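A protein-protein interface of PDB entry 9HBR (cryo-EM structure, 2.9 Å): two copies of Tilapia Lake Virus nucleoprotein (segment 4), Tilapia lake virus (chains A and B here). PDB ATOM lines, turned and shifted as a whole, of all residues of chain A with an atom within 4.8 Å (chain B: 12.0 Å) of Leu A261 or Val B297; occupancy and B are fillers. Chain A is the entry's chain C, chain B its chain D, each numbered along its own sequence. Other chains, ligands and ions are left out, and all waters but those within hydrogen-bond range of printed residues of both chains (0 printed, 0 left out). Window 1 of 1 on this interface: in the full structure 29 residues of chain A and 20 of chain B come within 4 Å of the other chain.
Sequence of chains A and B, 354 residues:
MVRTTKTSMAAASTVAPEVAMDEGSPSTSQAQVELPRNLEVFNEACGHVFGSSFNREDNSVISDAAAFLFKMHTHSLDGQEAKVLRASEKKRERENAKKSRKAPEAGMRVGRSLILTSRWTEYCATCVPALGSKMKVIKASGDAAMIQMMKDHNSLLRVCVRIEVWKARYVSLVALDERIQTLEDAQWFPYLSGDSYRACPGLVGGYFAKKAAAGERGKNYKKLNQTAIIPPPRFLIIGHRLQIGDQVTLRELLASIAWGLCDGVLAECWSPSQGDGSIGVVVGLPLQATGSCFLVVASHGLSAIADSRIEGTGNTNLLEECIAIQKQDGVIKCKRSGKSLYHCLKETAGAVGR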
ATOM      1  N   LEU A 176      13.278  18.895  24.840  1.00  0.00           N
ATOM      2  CA  LEU A 176      13.960  20.041  24.260  1.00  0.00           C
ATOM      3  C   LEU A 176      14.959  19.612  23.191  1.00  0.00           C
ATOM      4  O   LEU A 176      15.579  18.548  23.271  1.00  0.00           O
ATOM      5  CB  LEU A 176      14.677  20.841  25.346  1.00  0.00           C
ATOM      6  CG  LEU A 176      13.762  21.527  26.363  1.00  0.00           C
ATOM      7  CD1 LEU A 176      14.587  22.200  27.444  1.00  0.00           C
ATOM      8  CD2 LEU A 176      12.844  22.531  25.684  1.00  0.00           C
ATOM      9  N   ILE A 180      19.598  23.233  21.793  1.00  0.00           N
ATOM     10  CA  ILE A 180      19.306  24.261  22.783  1.00  0.00           C
ATOM     11  C   ILE A 180      20.062  23.895  24.055  1.00  0.00           C
ATOM     12  O   ILE A 180      19.626  23.040  24.829  1.00  0.00           O
ATOM     13  CB  ILE A 180      17.802  24.389  23.035  1.00  0.00           C
ATOM     14  CG1 ILE A 180      17.112  24.986  21.806  1.00  0.00           C
ATOM     15  CG2 ILE A 180      17.541  25.244  24.264  1.00  0.00           C
ATOM     16  CD1 ILE A 180      15.609  24.870  21.833  1.00  0.00           C
ATOM     17  N   LEU A 183      20.966  30.230  26.346  1.00  0.00           N
ATOM     18  CA  LEU A 183      19.931  31.164  25.915  1.00  0.00           C
ATOM     19  C   LEU A 183      20.150  31.602  24.474  1.00  0.00           C
ATOM     20  O   LEU A 183      19.185  31.829  23.735  1.00  0.00           O
ATOM     21  CB  LEU A 183      19.898  32.378  26.840  1.00  0.00           C
ATOM     22  CG  LEU A 183      19.390  32.154  28.263  1.00  0.00           C
ATOM     23  CD1 LEU A 183      19.397  33.466  29.018  1.00  0.00           C
ATOM     24  CD2 LEU A 183      18.005  31.546  28.269  1.00  0.00           C
ATOM     25  N   ALA A 186      18.639  28.957  22.489  1.00  0.00           N
ATOM     26  CA  ALA A 186      17.193  28.945  22.669  1.00  0.00           C
ATOM     27  C   ALA A 186      16.516  30.124  21.989  1.00  0.00           C
ATOM     28  O   ALA A 186      15.300  30.089  21.781  1.00  0.00           O
ATOM     29  CB  ALA A 186      16.848  28.945  24.158  1.00  0.00           C
ATOM     30  N   GLN A 226       8.562  34.305  19.055  1.00  0.00           N
ATOM     31  CA  GLN A 226       8.514  32.941  19.562  1.00  0.00           C
ATOM     32  C   GLN A 226       7.215  32.629  20.289  1.00  0.00           C
ATOM     33  O   GLN A 226       6.886  31.453  20.459  1.00  0.00           O
ATOM     34  CB  GLN A 226       9.688  32.689  20.502  1.00  0.00           C
ATOM     35  CG  GLN A 226      11.027  32.583  19.810  1.00  0.00           C
ATOM     36  CD  GLN A 226      12.074  31.936  20.684  1.00  0.00           C
ATOM     37  OE1 GLN A 226      12.056  32.084  21.902  1.00  0.00           O
ATOM     38  NE2 GLN A 226      12.997  31.216  20.065  1.00  0.00           N
ATOM     39  N   TRP A 259       6.119  27.983  24.405  1.00  0.00           N
ATOM     40  CA  TRP A 259       6.810  26.715  24.203  1.00  0.00           C
ATOM     41  C   TRP A 259       7.446  26.296  25.526  1.00  0.00           C
ATOM     42  O   TRP A 259       7.176  26.874  26.582  1.00  0.00           O
ATOM     43  CB  TRP A 259       7.826  26.815  23.058  1.00  0.00           C
ATOM     44  CG  TRP A 259       8.880  27.855  23.220  1.00  0.00           C
ATOM     45  CD1 TRP A 259       8.701  29.200  23.280  1.00  0.00           C
ATOM     46  CD2 TRP A 259      10.290  27.634  23.319  1.00  0.00           C
ATOM     47  NE1 TRP A 259       9.908  29.833  23.415  1.00  0.00           N
ATOM     48  CE2 TRP A 259      10.901  28.891  23.441  1.00  0.00           C
ATOM     49  CE3 TRP A 259      11.094  26.492  23.318  1.00  0.00           C
ATOM     50  CZ2 TRP A 259      12.275  29.042  23.565  1.00  0.00           C
ATOM     51  CZ3 TRP A 259      12.458  26.643  23.438  1.00  0.00           C
ATOM     52  CH2 TRP A 259      13.035  27.908  23.559  1.00  0.00           C
ATOM     53  N   GLY A 260       8.299  25.272  25.463  1.00  0.00           N
ATOM     54  CA  GLY A 260       8.738  24.602  26.677  1.00  0.00           C
ATOM     55  C   GLY A 260       9.549  25.485  27.604  1.00  0.00           C
ATOM     56  O   GLY A 260       9.366  25.450  28.821  1.00  0.00           O
ATOM     57  N   LEU A 261      10.461  26.278  27.052  1.00  0.00           N
ATOM     58  CA  LEU A 261      11.364  27.078  27.867  1.00  0.00           C
ATOM     59  C   LEU A 261      10.766  28.411  28.294  1.00  0.00           C
ATOM     60  O   LEU A 261      11.457  29.202  28.940  1.00  0.00           O
ATOM     61  CB  LEU A 261      12.679  27.320  27.122  1.00  0.00           C
ATOM     62  CG  LEU A 261      13.631  26.125  27.016  1.00  0.00           C
ATOM     63  CD1 LEU A 261      14.860  26.501  26.212  1.00  0.00           C
ATOM     64  CD2 LEU A 261      14.031  25.608  28.383  1.00  0.00           C
ATOM     65  N   CYS A 262       9.515  28.687  27.945  1.00  0.00           N
ATOM     66  CA  CYS A 262       8.849  29.865  28.470  1.00  0.00           C
ATOM     67  C   CYS A 262       8.531  29.669  29.949  1.00  0.00           C
ATOM     68  O   CYS A 262       8.451  28.548  30.450  1.00  0.00           O
ATOM     69  CB  CYS A 262       7.571  30.152  27.685  1.00  0.00           C
ATOM     70  SG  CYS A 262       7.820  31.205  26.244  1.00  0.00           S
ATOM     71  N   ASP A 263       8.346  30.785  30.650  1.00  0.00           N
ATOM     72  CA  ASP A 263       8.132  30.735  32.090  1.00  0.00           C
ATOM     73  C   ASP A 263       6.859  29.968  32.424  1.00  0.00           C
ATOM     74  O   ASP A 263       5.865  30.031  31.698  1.00  0.00           O
ATOM     75  CB  ASP A 263       8.056  32.150  32.659  1.00  0.00           C
ATOM     76  CG  ASP A 263       8.462  32.212  34.114  1.00  0.00           C
ATOM     77  OD1 ASP A 263       7.906  31.437  34.918  1.00  0.00           O
ATOM     78  OD2 ASP A 263       9.335  33.036  34.456  1.00  0.00           O
ATOM     79  N   SER A 340      10.902  27.199  33.891  1.00  0.00           N
ATOM     80  CA  SER A 340      10.353  27.015  32.560  1.00  0.00           C
ATOM     81  C   SER A 340       9.210  26.005  32.583  1.00  0.00           C
ATOM     82  O   SER A 340       9.099  25.169  33.482  1.00  0.00           O
ATOM     83  CB  SER A 340      11.437  26.554  31.589  1.00  0.00           C
ATOM     84  OG  SER A 340      12.336  25.659  32.213  1.00  0.00           O
ATOM     85  N   LEU A 341       8.343  26.102  31.573  1.00  0.00           N
ATOM     86  CA  LEU A 341       7.205  25.194  31.481  1.00  0.00           C
ATOM     87  C   LEU A 341       7.654  23.747  31.346  1.00  0.00           C
ATOM     88  O   LEU A 341       6.976  22.841  31.837  1.00  0.00           O
ATOM     89  CB  LEU A 341       6.327  25.582  30.293  1.00  0.00           C
ATOM     90  CG  LEU A 341       5.295  26.680  30.543  1.00  0.00           C
ATOM     91  CD1 LEU A 341       4.765  27.203  29.226  1.00  0.00           C
ATOM     92  CD2 LEU A 341       4.162  26.172  31.412  1.00  0.00           C
ATOM     93  N   ARG B 217      25.543  22.467  14.186  1.00  0.00           N
ATOM     94  CA  ARG B 217      24.709  21.439  14.797  1.00  0.00           C
ATOM     95  C   ARG B 217      23.518  21.176  13.885  1.00  0.00           C
ATOM     96  O   ARG B 217      22.677  22.057  13.685  1.00  0.00           O
ATOM     97  CB  ARG B 217      24.247  21.873  16.185  1.00  0.00           C
ATOM     98  CG  ARG B 217      25.371  22.157  17.162  1.00  0.00           C
ATOM     99  CD  ARG B 217      24.817  22.531  18.522  1.00  0.00           C
ATOM    100  NE  ARG B 217      25.867  22.891  19.465  1.00  0.00           N
ATOM    101  CZ  ARG B 217      25.647  23.311  20.703  1.00  0.00           C
ATOM    102  NH1 ARG B 217      24.422  23.431  21.186  1.00  0.00           N
ATOM    103  NH2 ARG B 217      26.685  23.618  21.478  1.00  0.00           N
ATOM    104  N   LYS B 223      23.810  15.388  21.999  1.00  0.00           N
ATOM    105  CA  LYS B 223      24.592  15.958  23.083  1.00  0.00           C
ATOM    106  C   LYS B 223      25.175  14.854  23.954  1.00  0.00           C
ATOM    107  O   LYS B 223      24.643  13.743  24.025  1.00  0.00           O
ATOM    108  CB  LYS B 223      23.739  16.905  23.930  1.00  0.00           C
ATOM    109  CG  LYS B 223      22.591  16.240  24.678  1.00  0.00           C
ATOM    110  CD  LYS B 223      22.387  16.855  26.053  1.00  0.00           C
ATOM    111  CE  LYS B 223      20.911  17.022  26.371  1.00  0.00           C
ATOM    112  NZ  LYS B 223      20.685  17.454  27.778  1.00  0.00           N
ATOM    113  N   GLN B 288      16.424  12.285  36.457  1.00  0.00           N
ATOM    114  CA  GLN B 288      17.040  13.355  35.675  1.00  0.00           C
ATOM    115  C   GLN B 288      18.464  12.992  35.265  1.00  0.00           C
ATOM    116  O   GLN B 288      19.340  13.853  35.182  1.00  0.00           O
ATOM    117  CB  GLN B 288      17.024  14.678  36.447  1.00  0.00           C
ATOM    118  CG  GLN B 288      16.019  15.684  35.924  1.00  0.00           C
ATOM    119  CD  GLN B 288      15.886  16.891  36.828  1.00  0.00           C
ATOM    120  OE1 GLN B 288      16.588  17.887  36.659  1.00  0.00           O
ATOM    121  NE2 GLN B 288      14.983  16.806  37.797  1.00  0.00           N
ATOM    122  N   GLY B 291      18.865  15.098  30.086  1.00  0.00           N
ATOM    123  CA  GLY B 291      17.864  16.084  29.722  1.00  0.00           C
ATOM    124  C   GLY B 291      17.509  17.057  30.824  1.00  0.00           C
ATOM    125  O   GLY B 291      16.323  17.327  31.048  1.00  0.00           O
ATOM    126  N   SER B 292      18.507  17.586  31.526  1.00  0.00           N
ATOM    127  CA  SER B 292      18.300  18.596  32.559  1.00  0.00           C
ATOM    128  C   SER B 292      18.601  19.963  31.956  1.00  0.00           C
ATOM    129  O   SER B 292      19.754  20.265  31.633  1.00  0.00           O
ATOM    130  CB  SER B 292      19.182  18.327  33.775  1.00  0.00           C
ATOM    131  OG  SER B 292      19.293  16.940  34.035  1.00  0.00           O
ATOM    132  N   CYS B 293      17.565  20.783  31.799  1.00  0.00           N
ATOM    133  CA  CYS B 293      17.699  22.147  31.307  1.00  0.00           C
ATOM    134  C   CYS B 293      17.058  23.096  32.306  1.00  0.00           C
ATOM    135  O   CYS B 293      15.936  22.856  32.762  1.00  0.00           O
ATOM    136  CB  CYS B 293      17.050  22.307  29.931  1.00  0.00           C
ATOM    137  SG  CYS B 293      17.525  23.822  29.070  1.00  0.00           S
ATOM    138  N   PHE B 294      17.771  24.166  32.643  1.00  0.00           N
ATOM    139  CA  PHE B 294      17.322  25.142  33.628  1.00  0.00           C
ATOM    140  C   PHE B 294      17.329  26.541  33.035  1.00  0.00           C
ATOM    141  O   PHE B 294      17.734  27.511  33.681  1.00  0.00           O
ATOM    142  CB  PHE B 294      18.188  25.077  34.883  1.00  0.00           C
ATOM    143  CG  PHE B 294      18.193  23.727  35.536  1.00  0.00           C
ATOM    144  CD1 PHE B 294      17.185  23.361  36.408  1.00  0.00           C
ATOM    145  CD2 PHE B 294      19.199  22.818  35.264  1.00  0.00           C
ATOM    146  CE1 PHE B 294      17.184  22.119  37.003  1.00  0.00           C
ATOM    147  CE2 PHE B 294      19.201  21.574  35.856  1.00  0.00           C
ATOM    148  CZ  PHE B 294      18.194  21.224  36.726  1.00  0.00           C
ATOM    149  N   LEU B 295      16.879  26.662  31.791  1.00  0.00           N
ATOM    150  CA  LEU B 295      16.750  27.941  31.114  1.00  0.00           C
ATOM    151  C   LEU B 295      15.307  28.417  31.179  1.00  0.00           C
ATOM    152  O   LEU B 295      14.370  27.617  31.223  1.00  0.00           O
ATOM    153  CB  LEU B 295      17.181  27.839  29.650  1.00  0.00           C
ATOM    154  CG  LEU B 295      18.585  27.314  29.362  1.00  0.00           C
ATOM    155  CD1 LEU B 295      18.852  27.354  27.871  1.00  0.00           C
ATOM    156  CD2 LEU B 295      19.628  28.114  30.116  1.00  0.00           C
ATOM    157  N   VAL B 296      15.139  29.736  31.193  1.00  0.00           N
ATOM    158  CA  VAL B 296      13.822  30.348  31.073  1.00  0.00           C
ATOM    159  C   VAL B 296      13.953  31.546  30.146  1.00  0.00           C
ATOM    160  O   VAL B 296      14.448  32.602  30.549  1.00  0.00           O
ATOM    161  CB  VAL B 296      13.258  30.762  32.442  1.00  0.00           C
ATOM    162  CG1 VAL B 296      11.785  31.095  32.326  1.00  0.00           C
ATOM    163  CG2 VAL B 296      13.477  29.661  33.462  1.00  0.00           C
ATOM    164  N   VAL B 297      13.522  31.387  28.895  1.00  0.00           N
ATOM    165  CA  VAL B 297      13.676  32.455  27.918  1.00  0.00           C
ATOM    166  C   VAL B 297      12.745  33.612  28.263  1.00  0.00           C
ATOM    167  O   VAL B 297      11.683  33.433  28.874  1.00  0.00           O
ATOM    168  CB  VAL B 297      13.411  31.937  26.493  1.00  0.00           C
ATOM    169  CG1 VAL B 297      14.465  30.920  26.099  1.00  0.00           C
ATOM    170  CG2 VAL B 297      12.015  31.342  26.382  1.00  0.00           C
ATOM    171  N   ALA B 298      13.153  34.815  27.870  1.00  0.00           N
ATOM    172  CA  ALA B 298      12.344  36.004  28.091  1.00  0.00           C
ATOM    173  C   ALA B 298      11.120  35.975  27.190  1.00  0.00           C
ATOM    174  O   ALA B 298      11.224  35.673  25.997  1.00  0.00           O
ATOM    175  CB  ALA B 298      13.166  37.264  27.824  1.00  0.00           C
ATOM    176  N   SER B 299       9.959  36.285  27.758  1.00  0.00           N
ATOM    177  CA  SER B 299       8.727  36.290  26.989  1.00  0.00           C
ATOM    178  C   SER B 299       7.662  37.049  27.761  1.00  0.00           C
ATOM    179  O   SER B 299       7.647  37.041  28.993  1.00  0.00           O
ATOM    180  CB  SER B 299       8.252  34.864  26.691  1.00  0.00           C
ATOM    181  OG  SER B 299       7.537  34.327  27.788  1.00  0.00           O
ATOM    182  N   HIS B 300       6.770  37.703  27.020  1.00  0.00           N
ATOM    183  CA  HIS B 300       5.635  38.413  27.605  1.00  0.00           C
ATOM    184  C   HIS B 300       6.095  39.430  28.647  1.00  0.00           C
ATOM    185  O   HIS B 300       5.458  39.615  29.685  1.00  0.00           O
ATOM    186  CB  HIS B 300       4.637  37.432  28.215  1.00  0.00           C
ATOM    187  CG  HIS B 300       4.214  36.346  27.280  1.00  0.00           C
ATOM    188  ND1 HIS B 300       4.798  35.098  27.276  1.00  0.00           N
ATOM    189  CD2 HIS B 300       3.262  36.318  26.318  1.00  0.00           C
ATOM    190  CE1 HIS B 300       4.226  34.350  26.352  1.00  0.00           C
ATOM    191  NE2 HIS B 300       3.291  35.066  25.756  1.00  0.00           N
ATOM    192  N   GLY B 301       7.206  40.100  28.366  1.00  0.00           N
ATOM    193  CA  GLY B 301       7.734  41.102  29.263  1.00  0.00           C
ATOM    194  C   GLY B 301       8.585  40.569  30.391  1.00  0.00           C
ATOM    195  O   GLY B 301       9.089  41.367  31.191  1.00  0.00           O
ATOM    196  N   LEU B 302       8.762  39.256  30.487  1.00  0.00           N
ATOM    197  CA  LEU B 302       9.624  38.677  31.502  1.00  0.00           C
ATOM    198  C   LEU B 302      11.084  38.764  31.064  1.00  0.00           C
ATOM    199  O   LEU B 302      11.403  39.138  29.934  1.00  0.00           O
ATOM    200  CB  LEU B 302       9.228  37.228  31.769  1.00  0.00           C
ATOM    201  CG  LEU B 302       7.837  37.039  32.372  1.00  0.00           C
ATOM    202  CD1 LEU B 302       7.325  35.637  32.101  1.00  0.00           C
ATOM    203  CD2 LEU B 302       7.857  37.327  33.859  1.00  0.00           C
ATOM    204  N   SER B 303      11.979  38.418  31.982  1.00  0.00           N
ATOM    205  CA  SER B 303      13.412  38.478  31.743  1.00  0.00           C
ATOM    206  C   SER B 303      13.993  37.071  31.717  1.00  0.00           C
ATOM    207  O   SER B 303      13.545  36.188  32.454  1.00  0.00           O
ATOM    208  CB  SER B 303      14.111  39.314  32.817  1.00  0.00           C
ATOM    209  OG  SER B 303      15.270  39.944  32.298  1.00  0.00           O
ATOM    210  N   ALA B 304      14.992  36.870  30.864  1.00  0.00           N
ATOM    211  CA  ALA B 304      15.600  35.560  30.714  1.00  0.00           C
ATOM    212  C   ALA B 304      16.348  35.161  31.980  1.00  0.00           C
ATOM    213  O   ALA B 304      16.799  36.006  32.758  1.00  0.00           O
ATOM    214  CB  ALA B 304      16.557  35.550  29.524  1.00  0.00           C
ATOM    215  N   ILE B 305      16.467  33.852  32.187  1.00  0.00           N
ATOM    216  CA  ILE B 305      17.200  33.285  33.312  1.00  0.00           C
ATOM    217  C   ILE B 305      18.169  32.251  32.760  1.00  0.00           C
ATOM    218  O   ILE B 305      17.746  31.283  32.118  1.00  0.00           O
ATOM    219  CB  ILE B 305      16.261  32.649  34.348  1.00  0.00           C
ATOM    220  CG1 ILE B 305      15.389  33.723  35.000  1.00  0.00           C
ATOM    221  CG2 ILE B 305      17.060  31.903  35.399  1.00  0.00           C
ATOM    222  CD1 ILE B 305      14.208  33.174  35.757  1.00  0.00           C
ATOM    223  N   ALA B 306      19.464  32.451  33.007  1.00  0.00           N
ATOM    224  CA  ALA B 306      20.459  31.506  32.514  1.00  0.00           C
ATOM    225  C   ALA B 306      20.461  30.214  33.322  1.00  0.00           C
ATOM    226  O   ALA B 306      20.850  29.163  32.804  1.00  0.00           O
ATOM    227  CB  ALA B 306      21.846  32.144  32.537  1.00  0.00           C
ATOM    228  N   ASP B 307      20.041  30.270  34.584  1.00  0.00           N
ATOM    229  CA  ASP B 307      20.011  29.084  35.436  1.00  0.00           C
ATOM    230  C   ASP B 307      18.968  29.312  36.519  1.00  0.00           C
ATOM    231  O   ASP B 307      19.115  30.221  37.339  1.00  0.00           O
ATOM    232  CB  ASP B 307      21.384  28.811  36.043  1.00  0.00           C
ATOM    233  CG  ASP B 307      21.486  27.429  36.661  1.00  0.00           C
ATOM    234  OD1 ASP B 307      20.543  27.020  37.368  1.00  0.00           O
ATOM    235  OD2 ASP B 307      22.511  26.752  36.440  1.00  0.00           O
ATOM    236  N   SER B 308      17.919  28.489  36.520  1.00  0.00           N
ATOM    237  CA  SER B 308      16.880  28.623  37.536  1.00  0.00           C
ATOM    238  C   SER B 308      17.428  28.337  38.927  1.00  0.00           C
ATOM    239  O   SER B 308      17.042  28.993  39.900  1.00  0.00           O
ATOM    240  CB  SER B 308      15.718  27.686  37.221  1.00  0.00           C
ATOM    241  OG  SER B 308      15.528  27.570  35.825  1.00  0.00           O
ATOM    242  N   ARG B 309      18.321  27.353  39.042  1.00  0.00           N
ATOM    243  CA  ARG B 309      18.860  26.981  40.346  1.00  0.00           C
ATOM    244  C   ARG B 309      19.604  28.149  40.983  1.00  0.00           C
ATOM    245  O   ARG B 309      19.335  28.526  42.128  1.00  0.00           O
ATOM    246  CB  ARG B 309      19.785  25.773  40.196  1.00  0.00           C
ATOM    247  CG  ARG B 309      19.113  24.541  39.603  1.00  0.00           C
ATOM    248  CD  ARG B 309      20.124  23.509  39.108  1.00  0.00           C
ATOM    249  NE  ARG B 309      21.148  24.085  38.243  1.00  0.00           N
ATOM    250  CZ  ARG B 309      21.996  23.373  37.514  1.00  0.00           C
ATOM    251  NH1 ARG B 309      21.972  22.052  37.518  1.00  0.00           N
ATOM    252  NH2 ARG B 309      22.889  24.004  36.757  1.00  0.00           N
ATOM    253  N   GLU B 311      19.487  31.342  40.243  1.00  0.00           N
ATOM    254  CA  GLU B 311      18.556  32.442  40.467  1.00  0.00           C
ATOM    255  C   GLU B 311      17.787  32.237  41.765  1.00  0.00           C
ATOM    256  O   GLU B 311      17.532  31.104  42.173  1.00  0.00           O
ATOM    257  CB  GLU B 311      17.582  32.567  39.295  1.00  0.00           C
ATOM    258  CG  GLU B 311      17.262  33.996  38.906  1.00  0.00           C
ATOM    259  CD  GLU B 311      18.448  34.714  38.294  1.00  0.00           C
ATOM    260  OE1 GLU B 311      19.313  35.194  39.057  1.00  0.00           O
ATOM    261  OE2 GLU B 311      18.513  34.803  37.050  1.00  0.00           O
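Printed residues of chain B that touch a printed residue of chain A: Cys B293, Leu B295, Val B296, Val B297, Ser B299, Leu B302, Ala B304 and Ile B305. Hydrophobic or aromatic side chains of chain B within 4 Å of the printed part of chain A: Leu B295, Val B296, Val B297, Leu B302 and Ala B304. Among the printed residues, 16 pairs touch across the chains.
Leu A183 touches Leu B295 (N to CD1, 3.9 Å). Ala B304 touches Leu A183 (CB to CD1, 3.6 Å). Leu A183 touches Ile B305 (CD2 to O, 3.9 Å). Ala A186 touches Val B297 (CB to CG1, 3.7 Å). CD2 of Leu A261 touches SG of Cys B293, at 3.98 Å. CD2 of Leu A261 touches O of Leu B295 (3.5 Å). Val B296 touches Leu A261 (CA to O, 3.4 Å). N of Cys A262 touches CG2 of Val B297, at 3.97 Å. Leu B302 touches Asp A263 (CD1 to CB, 3.6 Å). Val B296 touches Ser A340 (CG2 to N, 3.6 Å).
Val B297 touches just these residues of chain A: Ala A186 (3.7 Å), Trp A259 (3.6 Å), Leu A261 (3.0 Å) and Cys A262 (3.97 Å). No residue of chain B comes within 4 Å of Ile A180. Leu A183 touches just these residues of chain B: Leu B295, Ala B304 and Ile B305. Of chain B, only Val B297 (3.7 Å) comes within 4 Å of Ala A186. No residue of chain B comes within 4 Å of Gly A260. Cys A262 touches just these residues of chain B: Val B297 and Ser B299. Of the printed residues of chain B, Asp A263 touches Val B296 and Leu B302. No residue of chain B comes within 4 Å of Leu A341. Of the printed residues of chain A, Ile B305 touches Leu A183 (3.9 Å). Of the printed residues of chain A, Cys B293 touches Leu A176 and Leu A261. Phe B294 touches none of the printed residues of chain A. Gly B301 touches none of the printed residues of chain A. The nearest residue of chain A that does not touch Val B297 is Leu A183 (4.2 Å). The nearest printed residue of chain A that does not touch Cys B293 is Ser A340 (4.6 Å).
NE2 of Gln A226 is in hydrogen-bond range of O of Ala A186, at 3.1 Å. O of Cys A262 is in hydrogen-bond range of N of Leu A341. The side-chain amide oxygen (OE1) of Gln A226 is in hydrogen-bond range of the indole nitrogen (NE1) of Trp A259. The side-chain hydroxyl of Ser B299 lies within hydrogen-bond range of a ring nitrogen (ND1) of His B300, at 2.9 Å. NE1 of Trp A259 sits close to SG of Cys A262 (3.8 Å). The backbone carbonyl oxygen of Val B296 lies within hydrogen-bond range of the backbone NH of Ile B305 (2.9 Å).
No position is printed for both chains. Of the 16 pairs that touch across the chains among the printed residues, none has its exchanged pair printed and touching as well.
O of Leu A261 is in hydrogen-bond range of N of Val B297 (3.0 Å). The side-chain hydroxyl (OG) of Ser A340 is in hydrogen-bond range of the backbone carbonyl oxygen (O) of Leu B295 (3.0 Å). The side-chain hydroxyl (OG) of Ser B299 lies within hydrogen-bond range of the side-chain sulfur (SG) of Cys A262 (3.5 Å).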
